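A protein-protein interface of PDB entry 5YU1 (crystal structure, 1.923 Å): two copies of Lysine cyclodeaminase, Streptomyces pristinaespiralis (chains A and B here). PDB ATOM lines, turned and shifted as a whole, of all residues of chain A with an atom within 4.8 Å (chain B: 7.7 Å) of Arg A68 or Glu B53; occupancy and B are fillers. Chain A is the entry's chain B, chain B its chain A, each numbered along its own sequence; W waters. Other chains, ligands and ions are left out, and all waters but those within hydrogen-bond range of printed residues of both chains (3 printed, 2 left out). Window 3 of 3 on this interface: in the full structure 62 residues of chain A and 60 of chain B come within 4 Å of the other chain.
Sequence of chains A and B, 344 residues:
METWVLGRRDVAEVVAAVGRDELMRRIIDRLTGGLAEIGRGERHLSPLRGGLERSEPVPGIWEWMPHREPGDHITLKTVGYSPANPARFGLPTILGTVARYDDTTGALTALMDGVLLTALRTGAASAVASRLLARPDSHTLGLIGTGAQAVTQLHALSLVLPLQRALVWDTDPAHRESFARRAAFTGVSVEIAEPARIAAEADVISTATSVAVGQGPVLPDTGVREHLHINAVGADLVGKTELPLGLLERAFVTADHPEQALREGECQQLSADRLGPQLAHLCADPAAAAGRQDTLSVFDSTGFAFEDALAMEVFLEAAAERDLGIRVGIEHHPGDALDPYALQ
The backbone carbonyl oxygen (O) of Asp A103 is in hydrogen-bond range of the guanidinium group (NH1) of Arg B54, 2.7 Å away.
The backbone carbonyl oxygen of Glu B53 lies within hydrogen-bond range of the guanidinium group of Arg A68, at 3.4 Å.
N of Gly B60 is in hydrogen-bond range of O of Arg B54.
The guanidinium group (NH2) of Arg B54 is in hydrogen-bond range of the backbone carbonyl oxygen (O) of Ile B61, 3.0 Å away.
N of Gly A71 is in hydrogen-bond range of OD2 of Asp A103 (2.7 Å).
The guanidinium group (NE) of Arg A68 is in salt-bridge range of the side-chain carboxylate (OD1) of Asp A103.
The backbone NH of Leu B52 is in hydrogen-bond range of the backbone carbonyl oxygen of Trp B62.
CH2 of Trp B64 touches CG of Pro A66, 3.6 Å away.
Leu B52 touches Arg A68 (CD1 to CB, 3.96 Å).
Arg A68 touches Arg B54 (NE to CG, 3.4 Å).
Ile A74 touches Leu B52 (CG2 to CD1, 3.9 Å).
CB of Trp B62 touches CD1 of Ile A74, at 3.7 Å.
Of chain B, only Leu B52, Glu B53 and Arg B54 come within 4 Å of Arg A68.
Of the printed residues of chain A, Arg B54 touches Arg A68 and Asp A103.
Of the printed residues of chain B, Ile A74 touches Leu B52 (3.9 Å) and Trp B62 (3.7 Å).
Of the printed residues of chain A, Trp B62 touches Ile A74 (3.7 Å).
Pro B59 touches none of the printed residues of chain A.
The nearest residue of chain B that does not touch Arg A68 is Ser B55 (4.3 Å).
The nearest printed residue of chain A that does not touch Glu B53 is Asp A103 (6.1 Å).
Of the 9 printed residues of chain A, 4 touch a printed residue of chain B.
Printed residues of chain A that touch a printed residue of chain B: Pro A66, Arg A68, Ile A74 and Asp A103.
Hydrophobic or aromatic side chains of chain A within 4 Å of the printed part of chain B: Pro A66 and Ile A74.
Hydrophobic or aromatic side chains of chain B within 4 Å of the printed part of chain A: Leu B52, Trp B62 and Trp B64.
Along chain B the printed residues that touch a printed residue of chain A span positions 52 to 64.
No position is printed for both chains.
Of the 7 pairs that touch across the chains among the printed residues, none has its exchanged pair printed and touching as well.
Water W3 lies within hydrogen-bond range of the backbone carbonyl oxygen (O) of Glu B56 (2.6 Å), the guanidinium group (NH1) of Arg B54 (2.9 Å) and the backbone carbonyl oxygen (O) of Asp A103 (3.4 Å).
Water W1 bridges OD2 of Asp A103 (2.7 Å) and O of Glu B56 (3.0 Å).
Water W2 bridges the side-chain hydroxyl of Ser B55 and the guanidinium group of Arg A68.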
ATOM      1  N   PRO A  66      30.916  16.248  -7.550  1.00  0.00           N
ATOM      2  CA  PRO A  66      29.731  16.230  -6.685  1.00  0.00           C
ATOM      3  C   PRO A  66      28.935  17.525  -6.734  1.00  0.00           C
ATOM      4  O   PRO A  66      29.457  18.614  -7.003  1.00  0.00           O
ATOM      5  CB  PRO A  66      30.336  16.006  -5.289  1.00  0.00           C
ATOM      6  CG  PRO A  66      31.672  16.673  -5.357  1.00  0.00           C
ATOM      7  CD  PRO A  66      32.161  16.453  -6.789  1.00  0.00           C
ATOM      8  N   HIS A  67      27.628  17.384  -6.499  1.00  0.00           N
ATOM      9  CA  HIS A  67      26.762  18.541  -6.303  1.00  0.00           C
ATOM     10  C   HIS A  67      25.663  18.212  -5.301  1.00  0.00           C
ATOM     11  O   HIS A  67      25.025  17.159  -5.389  1.00  0.00           O
ATOM     12  CB  HIS A  67      26.097  19.023  -7.598  1.00  0.00           C
ATOM     13  CG  HIS A  67      25.237  20.231  -7.383  1.00  0.00           C
ATOM     14  ND1 HIS A  67      25.750  21.512  -7.358  1.00  0.00           N
ATOM     15  CD2 HIS A  67      23.912  20.351  -7.126  1.00  0.00           C
ATOM     16  CE1 HIS A  67      24.777  22.370  -7.105  1.00  0.00           C
ATOM     17  NE2 HIS A  67      23.652  21.691  -6.956  1.00  0.00           N
ATOM     18  N   ARG A  68      25.410  19.138  -4.378  1.00  0.00           N
ATOM     19  CA  ARG A  68      24.458  18.907  -3.300  1.00  0.00           C
ATOM     20  C   ARG A  68      23.262  19.835  -3.448  1.00  0.00           C
ATOM     21  O   ARG A  68      23.428  21.056  -3.570  1.00  0.00           O
ATOM     22  CB  ARG A  68      25.104  19.122  -1.928  1.00  0.00           C
ATOM     23  CG  ARG A  68      24.108  19.068  -0.781  1.00  0.00           C
ATOM     24  CD  ARG A  68      24.814  18.975   0.557  1.00  0.00           C
ATOM     25  NE  ARG A  68      23.854  18.780   1.640  1.00  0.00           N
ATOM     26  CZ  ARG A  68      23.552  19.704   2.550  1.00  0.00           C
ATOM     27  NH1 ARG A  68      24.143  20.896   2.508  1.00  0.00           N
ATOM     28  NH2 ARG A  68      22.651  19.438   3.494  1.00  0.00           N
ATOM     29  N   GLU A  69      22.062  19.248  -3.437  1.00  0.00           N
ATOM     30  CA  GLU A  69      20.822  19.996  -3.274  1.00  0.00           C
ATOM     31  C   GLU A  69      20.355  19.799  -1.834  1.00  0.00           C
ATOM     32  O   GLU A  69      19.772  18.752  -1.514  1.00  0.00           O
ATOM     33  CB  GLU A  69      19.755  19.527  -4.264  1.00  0.00           C
ATOM     34  CG  GLU A  69      20.032  19.971  -5.705  1.00  0.00           C
ATOM     35  CD  GLU A  69      19.890  21.479  -5.884  1.00  0.00           C
ATOM     36  OE1 GLU A  69      18.780  21.999  -5.640  1.00  0.00           O
ATOM     37  OE2 GLU A  69      20.886  22.149  -6.256  1.00  0.00           O
ATOM     38  N   PRO A  70      20.585  20.763  -0.943  1.00  0.00           N
ATOM     39  CA  PRO A  70      20.399  20.523   0.500  1.00  0.00           C
ATOM     40  C   PRO A  70      18.983  20.085   0.849  1.00  0.00           C
ATOM     41  O   PRO A  70      18.000  20.648   0.364  1.00  0.00           O
ATOM     42  CB  PRO A  70      20.743  21.880   1.123  1.00  0.00           C
ATOM     43  CG  PRO A  70      21.714  22.488   0.153  1.00  0.00           C
ATOM     44  CD  PRO A  70      21.258  22.044  -1.218  1.00  0.00           C
ATOM     45  N   GLY A  71      18.894  19.051   1.693  1.00  0.00           N
ATOM     46  CA  GLY A  71      17.630  18.465   2.077  1.00  0.00           C
ATOM     47  C   GLY A  71      17.014  17.538   1.052  1.00  0.00           C
ATOM     48  O   GLY A  71      16.033  16.856   1.367  1.00  0.00           O
ATOM     49  N   HIS A  73      18.983  15.817  -2.357  1.00  0.00           N
ATOM     50  CA  HIS A  73      19.882  14.757  -2.773  1.00  0.00           C
ATOM     51  C   HIS A  73      21.250  15.320  -3.125  1.00  0.00           C
ATOM     52  O   HIS A  73      21.429  16.522  -3.336  1.00  0.00           O
ATOM     53  CB  HIS A  73      19.301  13.986  -3.956  1.00  0.00           C
ATOM     54  CG  HIS A  73      18.771  14.869  -5.036  1.00  0.00           C
ATOM     55  ND1 HIS A  73      19.594  15.614  -5.854  1.00  0.00           N
ATOM     56  CD2 HIS A  73      17.502  15.150  -5.417  1.00  0.00           C
ATOM     57  CE1 HIS A  73      18.854  16.302  -6.706  1.00  0.00           C
ATOM     58  NE2 HIS A  73      17.583  16.038  -6.463  1.00  0.00           N
ATOM     59  N   ILE A  74      22.219  14.418  -3.153  1.00  0.00           N
ATOM     60  CA  ILE A  74      23.572  14.692  -3.609  1.00  0.00           C
ATOM     61  C   ILE A  74      23.769  13.939  -4.913  1.00  0.00           C
ATOM     62  O   ILE A  74      23.372  12.773  -5.026  1.00  0.00           O
ATOM     63  CB  ILE A  74      24.612  14.265  -2.558  1.00  0.00           C
ATOM     64  CG1 ILE A  74      24.382  15.024  -1.249  1.00  0.00           C
ATOM     65  CG2 ILE A  74      26.036  14.487  -3.079  1.00  0.00           C
ATOM     66  CD1 ILE A  74      25.254  14.556  -0.118  1.00  0.00           C
ATOM     67  N   ASP A 103      19.979  13.058   0.517  1.00  0.00           N
ATOM     68  CA  ASP A 103      20.766  13.975   1.331  1.00  0.00           C
ATOM     69  C   ASP A 103      20.504  13.778   2.815  1.00  0.00           C
ATOM     70  O   ASP A 103      21.389  14.034   3.638  1.00  0.00           O
ATOM     71  CB  ASP A 103      20.480  15.428   0.947  1.00  0.00           C
ATOM     72  CG  ASP A 103      21.385  16.407   1.681  1.00  0.00           C
ATOM     73  OD1 ASP A 103      22.614  16.265   1.564  1.00  0.00           O
ATOM     74  OD2 ASP A 103      20.874  17.309   2.382  1.00  0.00           O
ATOM     75  N   GLY B  51      34.611  16.230   1.037  1.00  0.00           N
ATOM     76  CA  GLY B  51      33.308  15.997   1.632  1.00  0.00           C
ATOM     77  C   GLY B  51      32.421  17.221   1.610  1.00  0.00           C
ATOM     78  O   GLY B  51      32.856  18.340   1.315  1.00  0.00           O
ATOM     79  N   LEU B  52      31.159  16.970   1.954  1.00  0.00           N
ATOM     80  CA  LEU B  52      30.080  17.951   1.998  1.00  0.00           C
ATOM     81  C   LEU B  52      29.407  17.853   3.358  1.00  0.00           C
ATOM     82  O   LEU B  52      28.863  16.797   3.704  1.00  0.00           O
ATOM     83  CB  LEU B  52      29.038  17.684   0.902  1.00  0.00           C
ATOM     84  CG  LEU B  52      29.318  17.955  -0.575  1.00  0.00           C
ATOM     85  CD1 LEU B  52      28.451  17.066  -1.445  1.00  0.00           C
ATOM     86  CD2 LEU B  52      29.045  19.407  -0.891  1.00  0.00           C
ATOM     87  N   GLU B  53      29.399  18.953   4.106  1.00  0.00           N
ATOM     88  CA  GLU B  53      28.729  18.993   5.402  1.00  0.00           C
ATOM     89  C   GLU B  53      27.219  19.120   5.242  1.00  0.00           C
ATOM     90  O   GLU B  53      26.730  19.821   4.356  1.00  0.00           O
ATOM     91  CB  GLU B  53      29.257  20.162   6.231  1.00  0.00           C
ATOM     92  CG  GLU B  53      30.704  20.001   6.635  1.00  0.00           C
ATOM     93  CD  GLU B  53      31.142  21.052   7.637  1.00  0.00           C
ATOM     94  OE1 GLU B  53      32.156  20.825   8.334  1.00  0.00           O
ATOM     95  OE2 GLU B  53      30.467  22.101   7.725  1.00  0.00           O
ATOM     96  N   ARG B  54      26.478  18.433   6.110  1.00  0.00           N
ATOM     97  CA  ARG B  54      25.021  18.482   6.122  1.00  0.00           C
ATOM     98  C   ARG B  54      24.580  18.806   7.540  1.00  0.00           C
ATOM     99  O   ARG B  54      25.068  18.195   8.493  1.00  0.00           O
ATOM    100  CB  ARG B  54      24.404  17.146   5.651  1.00  0.00           C
ATOM    101  CG  ARG B  54      24.708  16.777   4.193  1.00  0.00           C
ATOM    102  CD  ARG B  54      24.315  15.319   3.874  1.00  0.00           C
ATOM    103  NE  ARG B  54      25.052  14.456   4.750  1.00  0.00           N
ATOM    104  CZ  ARG B  54      24.609  13.337   5.306  1.00  0.00           C
ATOM    105  NH1 ARG B  54      23.393  12.843   5.071  1.00  0.00           N
ATOM    106  NH2 ARG B  54      25.425  12.708   6.112  1.00  0.00           N
ATOM    107  N   SER B  55      23.665  19.761   7.693  1.00  0.00           N
ATOM    108  CA  SER B  55      23.301  20.206   9.032  1.00  0.00           C
ATOM    109  C   SER B  55      22.059  19.525   9.588  1.00  0.00           C
ATOM    110  O   SER B  55      21.896  19.475  10.813  1.00  0.00           O
ATOM    111  CB  SER B  55      23.090  21.725   9.046  1.00  0.00           C
ATOM    112  OG  SER B  55      21.927  22.069   8.320  1.00  0.00           O
ATOM    113  N   GLU B  56      21.190  18.997   8.740  1.00  0.00           N
ATOM    114  CA  GLU B  56      19.950  18.420   9.233  1.00  0.00           C
ATOM    115  C   GLU B  56      19.891  16.921   8.940  1.00  0.00           C
ATOM    116  O   GLU B  56      20.470  16.459   7.952  1.00  0.00           O
ATOM    117  CB  GLU B  56      18.737  19.121   8.602  1.00  0.00           C
ATOM    118  CG  GLU B  56      18.525  20.545   9.109  1.00  0.00           C
ATOM    119  CD  GLU B  56      17.444  21.286   8.332  1.00  0.00           C
ATOM    120  OE1 GLU B  56      16.381  20.687   8.061  1.00  0.00           O
ATOM    121  OE2 GLU B  56      17.658  22.471   7.988  1.00  0.00           O
ATOM    122  N   VAL B  58      20.705  16.272  12.101  1.00  0.00           N
ATOM    123  CA  VAL B  58      21.832  16.652  12.953  1.00  0.00           C
ATOM    124  C   VAL B  58      23.058  16.756  12.052  1.00  0.00           C
ATOM    125  O   VAL B  58      23.046  16.242  10.922  1.00  0.00           O
ATOM    126  CB  VAL B  58      22.056  15.637  14.100  1.00  0.00           C
ATOM    127  CG1 VAL B  58      20.767  15.421  14.912  1.00  0.00           C
ATOM    128  CG2 VAL B  58      22.567  14.318  13.547  1.00  0.00           C
ATOM    129  N   PRO B  59      24.118  17.432  12.505  1.00  0.00           N
ATOM    130  CA  PRO B  59      25.286  17.625  11.631  1.00  0.00           C
ATOM    131  C   PRO B  59      25.903  16.307  11.190  1.00  0.00           C
ATOM    132  O   PRO B  59      26.209  15.430  12.004  1.00  0.00           O
ATOM    133  CB  PRO B  59      26.254  18.433  12.502  1.00  0.00           C
ATOM    134  CG  PRO B  59      25.357  19.192  13.429  1.00  0.00           C
ATOM    135  CD  PRO B  59      24.226  18.240  13.735  1.00  0.00           C
ATOM    136  N   GLY B  60      26.084  16.178   9.885  1.00  0.00           N
ATOM    137  CA  GLY B  60      26.744  15.014   9.335  1.00  0.00           C
ATOM    138  C   GLY B  60      27.592  15.417   8.156  1.00  0.00           C
ATOM    139  O   GLY B  60      27.792  16.615   7.910  1.00  0.00           O
ATOM    140  N   ILE B  61      28.109  14.434   7.427  1.00  0.00           N
ATOM    141  CA  ILE B  61      28.962  14.703   6.277  1.00  0.00           C
ATOM    142  C   ILE B  61      28.802  13.566   5.275  1.00  0.00           C
ATOM    143  O   ILE B  61      28.416  12.447   5.624  1.00  0.00           O
ATOM    144  CB  ILE B  61      30.443  14.905   6.706  1.00  0.00           C
ATOM    145  CG1 ILE B  61      31.251  15.583   5.586  1.00  0.00           C
ATOM    146  CG2 ILE B  61      31.086  13.590   7.169  1.00  0.00           C
ATOM    147  CD1 ILE B  61      32.550  16.239   6.065  1.00  0.00           C
ATOM    148  N   TRP B  62      29.064  13.874   4.014  1.00  0.00           N
ATOM    149  CA  TRP B  62      29.088  12.891   2.943  1.00  0.00           C
ATOM    150  C   TRP B  62      30.392  13.099   2.198  1.00  0.00           C
ATOM    151  O   TRP B  62      30.720  14.234   1.831  1.00  0.00           O
ATOM    152  CB  TRP B  62      27.867  13.048   2.021  1.00  0.00           C
ATOM    153  CG  TRP B  62      27.734  11.976   1.014  1.00  0.00           C
ATOM    154  CD1 TRP B  62      27.134  10.749   1.179  1.00  0.00           C
ATOM    155  CD2 TRP B  62      28.212  12.012  -0.332  1.00  0.00           C
ATOM    156  NE1 TRP B  62      27.220  10.025   0.008  1.00  0.00           N
ATOM    157  CE2 TRP B  62      27.874  10.779  -0.932  1.00  0.00           C
ATOM    158  CE3 TRP B  62      28.889  12.968  -1.090  1.00  0.00           C
ATOM    159  CZ2 TRP B  62      28.197  10.482  -2.255  1.00  0.00           C
ATOM    160  CZ3 TRP B  62      29.205  12.668  -2.407  1.00  0.00           C
ATOM    161  CH2 TRP B  62      28.860  11.440  -2.971  1.00  0.00           C
ATOM    162  N   GLU B  63      31.155  12.020   2.021  1.00  0.00           N
ATOM    163  CA  GLU B  63      32.539  12.117   1.599  1.00  0.00           C
ATOM    164  C   GLU B  63      32.815  11.183   0.426  1.00  0.00           C
ATOM    165  O   GLU B  63      32.148  10.159   0.237  1.00  0.00           O
ATOM    166  CB  GLU B  63      33.500  11.799   2.764  1.00  0.00           C
ATOM    167  CG  GLU B  63      33.433  12.836   3.896  1.00  0.00           C
ATOM    168  CD  GLU B  63      34.189  12.421   5.160  1.00  0.00           C
ATOM    169  OE1 GLU B  63      34.288  11.208   5.431  1.00  0.00           O
ATOM    170  OE2 GLU B  63      34.680  13.315   5.885  1.00  0.00           O
ATOM    171  N   TRP B  64      33.830  11.550  -0.353  1.00  0.00           N
ATOM    172  CA  TRP B  64      34.309  10.745  -1.468  1.00  0.00           C
ATOM    173  C   TRP B  64      35.801  10.508  -1.297  1.00  0.00           C
ATOM    174  O   TRP B  64      36.539  11.413  -0.896  1.00  0.00           O
ATOM    175  CB  TRP B  64      34.025  11.419  -2.819  1.00  0.00           C
ATOM    176  CG  TRP B  64      34.443  12.860  -2.871  1.00  0.00           C
ATOM    177  CD1 TRP B  64      35.633  13.355  -3.319  1.00  0.00           C
ATOM    178  CD2 TRP B  64      33.667  13.990  -2.465  1.00  0.00           C
ATOM    179  NE1 TRP B  64      35.645  14.726  -3.214  1.00  0.00           N
ATOM    180  CE2 TRP B  64      34.449  15.141  -2.701  1.00  0.00           C
ATOM    181  CE3 TRP B  64      32.387  14.142  -1.921  1.00  0.00           C
ATOM    182  CZ2 TRP B  64      33.993  16.428  -2.411  1.00  0.00           C
ATOM    183  CZ3 TRP B  64      31.934  15.428  -1.643  1.00  0.00           C
ATOM    184  CH2 TRP B  64      32.739  16.547  -1.884  1.00  0.00           C
ATOM    185  N   VAL B 213      30.775  17.932  17.186  1.00  0.00           N
ATOM    186  CA  VAL B 213      31.903  18.855  17.160  1.00  0.00           C
ATOM    187  C   VAL B 213      31.949  19.643  18.461  1.00  0.00           C
ATOM    188  O   VAL B 213      30.937  20.196  18.909  1.00  0.00           O
ATOM    189  CB  VAL B 213      31.791  19.786  15.936  1.00  0.00           C
ATOM    190  CG1 VAL B 213      32.726  20.997  16.069  1.00  0.00           C
ATOM    191  CG2 VAL B 213      32.090  19.018  14.652  1.00  0.00           C
ATOM    192  N   ASP B 236      34.700  12.467  11.564  1.00  0.00           N
ATOM    193  CA  ASP B 236      33.720  12.879  10.571  1.00  0.00           C
ATOM    194  C   ASP B 236      33.909  14.349  10.200  1.00  0.00           C
ATOM    195  O   ASP B 236      34.527  14.655   9.175  1.00  0.00           O
ATOM    196  CB  ASP B 236      32.294  12.605  11.069  1.00  0.00           C
ATOM    197  CG  ASP B 236      32.091  12.962  12.555  1.00  0.00           C
ATOM    198  OD1 ASP B 236      31.993  12.037  13.400  1.00  0.00           O
ATOM    199  OD2 ASP B 236      32.008  14.168  12.873  1.00  0.00           O
ATOM    200  N   LEU B 237      33.400  15.256  11.026  1.00  0.00           N
ATOM    201  CA  LEU B 237      33.482  16.687  10.767  1.00  0.00           C
ATOM    202  C   LEU B 237      34.786  17.271  11.310  1.00  0.00           C
ATOM    203  O   LEU B 237      35.330  16.804  12.314  1.00  0.00           O
ATOM    204  CB  LEU B 237      32.288  17.406  11.403  1.00  0.00           C
ATOM    205  CG  LEU B 237      30.898  16.990  10.902  1.00  0.00           C
ATOM    206  CD1 LEU B 237      29.801  17.201  11.950  1.00  0.00           C
ATOM    207  CD2 LEU B 237      30.574  17.776   9.641  1.00  0.00           C
ATOM    208  N   VAL B 238      35.288  18.311  10.634  1.00  0.00           N
ATOM    209  CA  VAL B 238      36.363  19.109  11.214  1.00  0.00           C
ATOM    210  C   VAL B 238      35.900  19.640  12.563  1.00  0.00           C
ATOM    211  O   VAL B 238      34.779  20.144  12.697  1.00  0.00           O
ATOM    212  CB  VAL B 238      36.765  20.245  10.259  1.00  0.00           C
ATOM    213  CG1 VAL B 238      37.684  21.250  10.960  1.00  0.00           C
ATOM    214  CG2 VAL B 238      37.423  19.671   9.006  1.00  0.00           C
ATOM    215  N   GLY B 239      36.747  19.501  13.583  1.00  0.00           N
ATOM    216  CA  GLY B 239      36.416  19.955  14.919  1.00  0.00           C
ATOM    217  C   GLY B 239      35.898  18.872  15.844  1.00  0.00           C
ATOM    218  O   GLY B 239      35.694  19.141  17.036  1.00  0.00           O
HETATM  219  O   HOH W   1      20.320  16.758   4.922  1.00  0.00           O
HETATM  220  O   HOH W   2      23.148  22.224   5.465  1.00  0.00           O
HETATM  221  O   HOH W   3      21.930  14.544   6.948  1.00  0.00           O
